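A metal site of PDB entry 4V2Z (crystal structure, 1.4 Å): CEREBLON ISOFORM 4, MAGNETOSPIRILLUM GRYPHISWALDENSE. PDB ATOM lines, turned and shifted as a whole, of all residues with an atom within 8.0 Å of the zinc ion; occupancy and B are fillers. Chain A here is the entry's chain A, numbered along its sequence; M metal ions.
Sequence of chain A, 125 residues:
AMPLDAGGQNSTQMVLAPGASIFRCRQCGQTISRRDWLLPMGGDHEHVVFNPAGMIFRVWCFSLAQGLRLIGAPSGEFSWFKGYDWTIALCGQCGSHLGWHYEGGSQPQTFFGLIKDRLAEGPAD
The side-chain sulfur (SG) of Cys 28 sits close to the backbone NH (N) of Gln 30 (3.5 Å).
The side-chain sulfur (SG) of Cys 28 sits close to the side-chain amide nitrogen (NE2) of Gln 93, at 3.2 Å.
N of Ser 96 sits close to SG of Cys 94 (3.5 Å).
N of Cys 25 is in hydrogen-bond range of O of Gln 30 (2.9 Å).
The side-chain sulfur of Cys 25 lies close to the backbone NH of Gln 27, at 3.4 Å.
N of Cys 91 is in hydrogen-bond range of O of Ser 96 (2.8 Å).
The side-chain sulfur (SG) of Cys 91 lies close to the backbone NH (N) of Gln 93, 3.5 Å away.
SG of Cys 28 binds the zinc ion (2.3 Å).
SG of Cys 94 binds the zinc ion (2.3 Å).
The zinc ion is bound by the side-chain sulfur (SG) of Cys 25 (2.3 Å).
The zinc ion is bound by SG of Cys 91.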
ATOM      1  N   ARG A  24      10.510  29.327   6.422  1.00  0.00           N
ATOM      2  CA  ARG A  24       9.643  28.366   5.795  1.00  0.00           C
ATOM      3  C   ARG A  24       8.221  28.884   5.801  1.00  0.00           C
ATOM      4  O   ARG A  24       7.835  29.666   6.650  1.00  0.00           O
ATOM      5  CB  ARG A  24       9.719  27.021   6.546  1.00  0.00           C
ATOM      6  CG  ARG A  24      11.043  26.363   6.432  1.00  0.00           C
ATOM      7  CD  ARG A  24      11.142  24.937   7.083  1.00  0.00           C
ATOM      8  NE  ARG A  24      12.361  24.309   6.891  1.00  0.00           N
ATOM      9  CZ  ARG A  24      12.786  23.794   5.782  1.00  0.00           C
ATOM     10  NH1 ARG A  24      11.899  23.621   4.803  1.00  0.00           N
ATOM     11  NH2 ARG A  24      14.012  23.267   5.662  1.00  0.00           N
ATOM     12  N   CYS A  25       7.349  28.368   4.939  1.00  0.00           N
ATOM     13  CA  CYS A  25       5.933  28.640   5.012  1.00  0.00           C
ATOM     14  C   CYS A  25       5.376  28.144   6.294  1.00  0.00           C
ATOM     15  O   CYS A  25       5.578  26.967   6.672  1.00  0.00           O
ATOM     16  CB  CYS A  25       5.232  27.984   3.849  1.00  0.00           C
ATOM     17  SG  CYS A  25       3.422  28.130   3.883  1.00  0.00           S
ATOM     18  N   ARG A  26       4.679  28.970   7.030  1.00  0.00           N
ATOM     19  CA  ARG A  26       4.085  28.592   8.253  1.00  0.00           C
ATOM     20  C   ARG A  26       3.071  27.483   8.159  1.00  0.00           C
ATOM     21  O   ARG A  26       2.818  26.780   9.147  1.00  0.00           O
ATOM     22  CB  ARG A  26       3.454  29.842   8.911  1.00  0.00           C
ATOM     23  CG  ARG A  26       2.789  29.677  10.232  1.00  0.00           C
ATOM     24  CD  ARG A  26       2.305  30.997  10.749  1.00  0.00           C
ATOM     25  NE  ARG A  26       1.551  30.803  11.902  1.00  0.00           N
ATOM     26  CZ  ARG A  26       0.968  31.725  12.655  1.00  0.00           C
ATOM     27  NH1 ARG A  26       1.148  33.044  12.371  1.00  0.00           N
ATOM     28  NH2 ARG A  26       0.244  31.386  13.699  1.00  0.00           N
ATOM     29  N   GLN A  27       2.355  27.465   7.038  1.00  0.00           N
ATOM     30  CA  GLN A  27       1.253  26.450   6.875  1.00  0.00           C
ATOM     31  C   GLN A  27       1.742  25.121   6.504  1.00  0.00           C
ATOM     32  O   GLN A  27       1.013  24.119   6.811  1.00  0.00           O
ATOM     33  CB  GLN A  27       0.226  26.958   5.887  1.00  0.00           C
ATOM     34  CG  GLN A  27      -0.360  28.246   6.367  1.00  0.00           C
ATOM     35  CD  GLN A  27      -0.902  28.195   7.799  1.00  0.00           C
ATOM     36  OE1 GLN A  27      -0.617  29.076   8.678  1.00  0.00           O
ATOM     37  NE2 GLN A  27      -1.701  27.245   8.046  1.00  0.00           N
ATOM     38  N   CYS A  28       2.922  24.951   5.924  1.00  0.00           N
ATOM     39  CA  CYS A  28       3.286  23.640   5.363  1.00  0.00           C
ATOM     40  C   CYS A  28       4.742  23.270   5.494  1.00  0.00           C
ATOM     41  O   CYS A  28       5.133  22.099   5.272  1.00  0.00           O
ATOM     42  CB  CYS A  28       2.815  23.484   3.929  1.00  0.00           C
ATOM     43  SG  CYS A  28       3.840  24.442   2.715  1.00  0.00           S
ATOM     44  N   GLY A  29       5.673  24.255   5.760  1.00  0.00           N
ATOM     45  CA  GLY A  29       7.005  23.926   5.740  1.00  0.00           C
ATOM     46  C   GLY A  29       7.879  24.130   4.556  1.00  0.00           C
ATOM     47  O   GLY A  29       9.107  23.999   4.621  1.00  0.00           O
ATOM     48  N   GLN A  30       7.290  24.484   3.438  1.00  0.00           N
ATOM     49  CA  GLN A  30       8.071  24.771   2.256  1.00  0.00           C
ATOM     50  C   GLN A  30       9.240  25.749   2.529  1.00  0.00           C
ATOM     51  O   GLN A  30       8.962  26.703   3.131  1.00  0.00           O
ATOM     52  CB  GLN A  30       7.150  25.408   1.231  1.00  0.00           C
ATOM     53  CG  GLN A  30       7.791  25.850  -0.049  1.00  0.00           C
ATOM     54  CD  GLN A  30       7.989  24.738  -1.041  1.00  0.00           C
ATOM     55  OE1 GLN A  30       8.411  23.624  -0.682  1.00  0.00           O
ATOM     56  NE2 GLN A  30       7.699  25.012  -2.300  1.00  0.00           N
ATOM     57  N   THR A  31      10.445  25.486   2.086  1.00  0.00           N
ATOM     58  CA  THR A  31      11.561  26.452   2.251  1.00  0.00           C
ATOM     59  C   THR A  31      11.270  27.701   1.354  1.00  0.00           C
ATOM     60  O   THR A  31      10.982  27.495   0.168  1.00  0.00           O
ATOM     61  CB  THR A  31      12.887  25.874   1.811  1.00  0.00           C
ATOM     62  OG1 THR A  31      13.027  24.516   2.318  1.00  0.00           O
ATOM     63  CG2 THR A  31      14.007  26.631   2.273  1.00  0.00           C
ATOM     64  N   ILE A  32      11.347  28.891   1.930  1.00  0.00           N
ATOM     65  CA  ILE A  32      11.077  30.140   1.242  1.00  0.00           C
ATOM     66  C   ILE A  32      12.224  31.119   1.149  1.00  0.00           C
ATOM     67  O   ILE A  32      12.556  31.623   0.075  1.00  0.00           O
ATOM     68  CB  ILE A  32       9.824  30.844   1.788  1.00  0.00           C
ATOM     69  CG1 ILE A  32       8.566  29.972   1.795  1.00  0.00           C
ATOM     70  CG2 ILE A  32       9.531  32.139   1.005  1.00  0.00           C
ATOM     71  CD1 ILE A  32       8.013  29.534   0.474  1.00  0.00           C
ATOM     72  N   GLY A  67      10.652  28.616  -3.759  1.00  0.00           N
ATOM     73  CA  GLY A  67       9.551  27.835  -3.274  1.00  0.00           C
ATOM     74  C   GLY A  67       8.174  28.469  -3.425  1.00  0.00           C
ATOM     75  O   GLY A  67       7.181  27.949  -2.871  1.00  0.00           O
ATOM     76  N   LEU A  90       2.423  33.075  -4.090  1.00  0.00           N
ATOM     77  CA  LEU A  90       1.861  31.997  -3.253  1.00  0.00           C
ATOM     78  C   LEU A  90       2.961  31.047  -2.829  1.00  0.00           C
ATOM     79  O   LEU A  90       3.928  30.887  -3.572  1.00  0.00           O
ATOM     80  CB  LEU A  90       0.757  31.253  -3.980  1.00  0.00           C
ATOM     81  CG  LEU A  90      -0.449  32.062  -4.523  1.00  0.00           C
ATOM     82  CD1 LEU A  90      -1.465  31.144  -5.203  1.00  0.00           C
ATOM     83  CD2 LEU A  90      -1.098  32.929  -3.472  1.00  0.00           C
ATOM     84  N   CYS A  91       2.810  30.431  -1.668  1.00  0.00           N
ATOM     85  CA  CYS A  91       3.602  29.226  -1.393  1.00  0.00           C
ATOM     86  C   CYS A  91       3.378  28.272  -2.562  1.00  0.00           C
ATOM     87  O   CYS A  91       2.264  27.909  -2.891  1.00  0.00           O
ATOM     88  CB  CYS A  91       3.122  28.583  -0.141  1.00  0.00           C
ATOM     89  SG  CYS A  91       4.065  27.067   0.265  1.00  0.00           S
ATOM     90  N   GLY A  92       4.465  27.788  -3.169  1.00  0.00           N
ATOM     91  CA  GLY A  92       4.367  26.877  -4.242  1.00  0.00           C
ATOM     92  C   GLY A  92       3.898  25.495  -3.897  1.00  0.00           C
ATOM     93  O   GLY A  92       3.454  24.736  -4.787  1.00  0.00           O
ATOM     94  N   GLN A  93       3.947  25.165  -2.631  1.00  0.00           N
ATOM     95  CA  GLN A  93       3.503  23.837  -2.164  1.00  0.00           C
ATOM     96  C   GLN A  93       2.021  23.920  -1.778  1.00  0.00           C
ATOM     97  O   GLN A  93       1.223  23.210  -2.402  1.00  0.00           O
ATOM     98  CB  GLN A  93       4.441  23.417  -1.012  1.00  0.00           C
ATOM     99  CG  GLN A  93       4.143  22.019  -0.439  1.00  0.00           C
ATOM    100  CD  GLN A  93       5.297  21.472   0.334  1.00  0.00           C
ATOM    101  OE1 GLN A  93       6.073  20.732  -0.230  1.00  0.00           O
ATOM    102  NE2 GLN A  93       5.445  21.900   1.543  1.00  0.00           N
ATOM    103  N   CYS A  94       1.665  24.821  -0.821  1.00  0.00           N
ATOM    104  CA  CYS A  94       0.320  24.786  -0.264  1.00  0.00           C
ATOM    105  C   CYS A  94      -0.635  25.859  -0.755  1.00  0.00           C
ATOM    106  O   CYS A  94      -1.839  25.784  -0.469  1.00  0.00           O
ATOM    107  CB  CYS A  94       0.354  24.755   1.235  1.00  0.00           C
ATOM    108  SG  CYS A  94       0.617  26.409   1.972  1.00  0.00           S
ATOM    109  N   GLY A  95      -0.099  26.871  -1.442  1.00  0.00           N
ATOM    110  CA  GLY A  95      -0.980  27.909  -1.984  1.00  0.00           C
ATOM    111  C   GLY A  95      -1.244  29.052  -1.045  1.00  0.00           C
ATOM    112  O   GLY A  95      -1.927  30.015  -1.471  1.00  0.00           O
ATOM    113  N   SER A  96      -0.738  29.038   0.153  1.00  0.00           N
ATOM    114  CA  SER A  96      -0.867  30.164   1.103  1.00  0.00           C
ATOM    115  C   SER A  96      -0.317  31.432   0.444  1.00  0.00           C
ATOM    116  O   SER A  96       0.710  31.419  -0.177  1.00  0.00           O
ATOM    117  CB  SER A  96      -0.066  29.835   2.341  1.00  0.00           C
ATOM    118  OG  SER A  96      -0.069  30.930   3.307  1.00  0.00           O
ATOM    119  N   HIS A  97      -1.027  32.543   0.637  1.00  0.00           N
ATOM    120  CA  HIS A  97      -0.549  33.792   0.129  1.00  0.00           C
ATOM    121  C   HIS A  97       0.549  34.330   1.020  1.00  0.00           C
ATOM    122  O   HIS A  97       0.341  34.788   2.159  1.00  0.00           O
ATOM    123  CB  HIS A  97      -1.646  34.826   0.063  1.00  0.00           C
ATOM    124  CG  HIS A  97      -1.201  36.125  -0.420  1.00  0.00           C
ATOM    125  ND1 HIS A  97      -1.845  37.287  -0.039  1.00  0.00           N
ATOM    126  CD2 HIS A  97      -0.173  36.489  -1.210  1.00  0.00           C
ATOM    127  CE1 HIS A  97      -1.229  38.305  -0.592  1.00  0.00           C
ATOM    128  NE2 HIS A  97      -0.213  37.850  -1.315  1.00  0.00           N
ATOM    129  N   LEU A  98       1.790  34.294   0.561  1.00  0.00           N
ATOM    130  CA  LEU A  98       2.952  34.688   1.322  1.00  0.00           C
ATOM    131  C   LEU A  98       3.433  36.109   1.075  1.00  0.00           C
ATOM    132  O   LEU A  98       4.148  36.612   1.908  1.00  0.00           O
ATOM    133  CB  LEU A  98       4.145  33.739   1.121  1.00  0.00           C
ATOM    134  CG  LEU A  98       3.874  32.296   1.581  1.00  0.00           C
ATOM    135  CD1 LEU A  98       5.056  31.394   1.499  1.00  0.00           C
ATOM    136  CD2 LEU A  98       3.299  32.170   2.937  1.00  0.00           C
ATOM    137  N   ARG A 118       3.361  35.064   8.132  1.00  0.00           N
ATOM    138  CA  ARG A 118       3.013  33.882   7.396  1.00  0.00           C
ATOM    139  C   ARG A 118       4.236  32.954   7.167  1.00  0.00           C
ATOM    140  O   ARG A 118       4.143  31.950   6.451  1.00  0.00           O
ATOM    141  CB  ARG A 118       2.306  34.319   6.122  1.00  0.00           C
ATOM    142  CG  ARG A 118       1.048  35.135   6.426  1.00  0.00           C
ATOM    143  CD  ARG A 118       0.175  35.341   5.164  1.00  0.00           C
ATOM    144  NE  ARG A 118      -0.921  36.274   5.448  1.00  0.00           N
ATOM    145  CZ  ARG A 118      -1.787  36.719   4.533  1.00  0.00           C
ATOM    146  NH1 ARG A 118      -1.667  36.360   3.267  1.00  0.00           N
ATOM    147  NH2 ARG A 118      -2.755  37.545   4.894  1.00  0.00           N
HETATM  148 ZN    ZN M   1       2.930  26.509   2.276  1.00  0.00          ZN
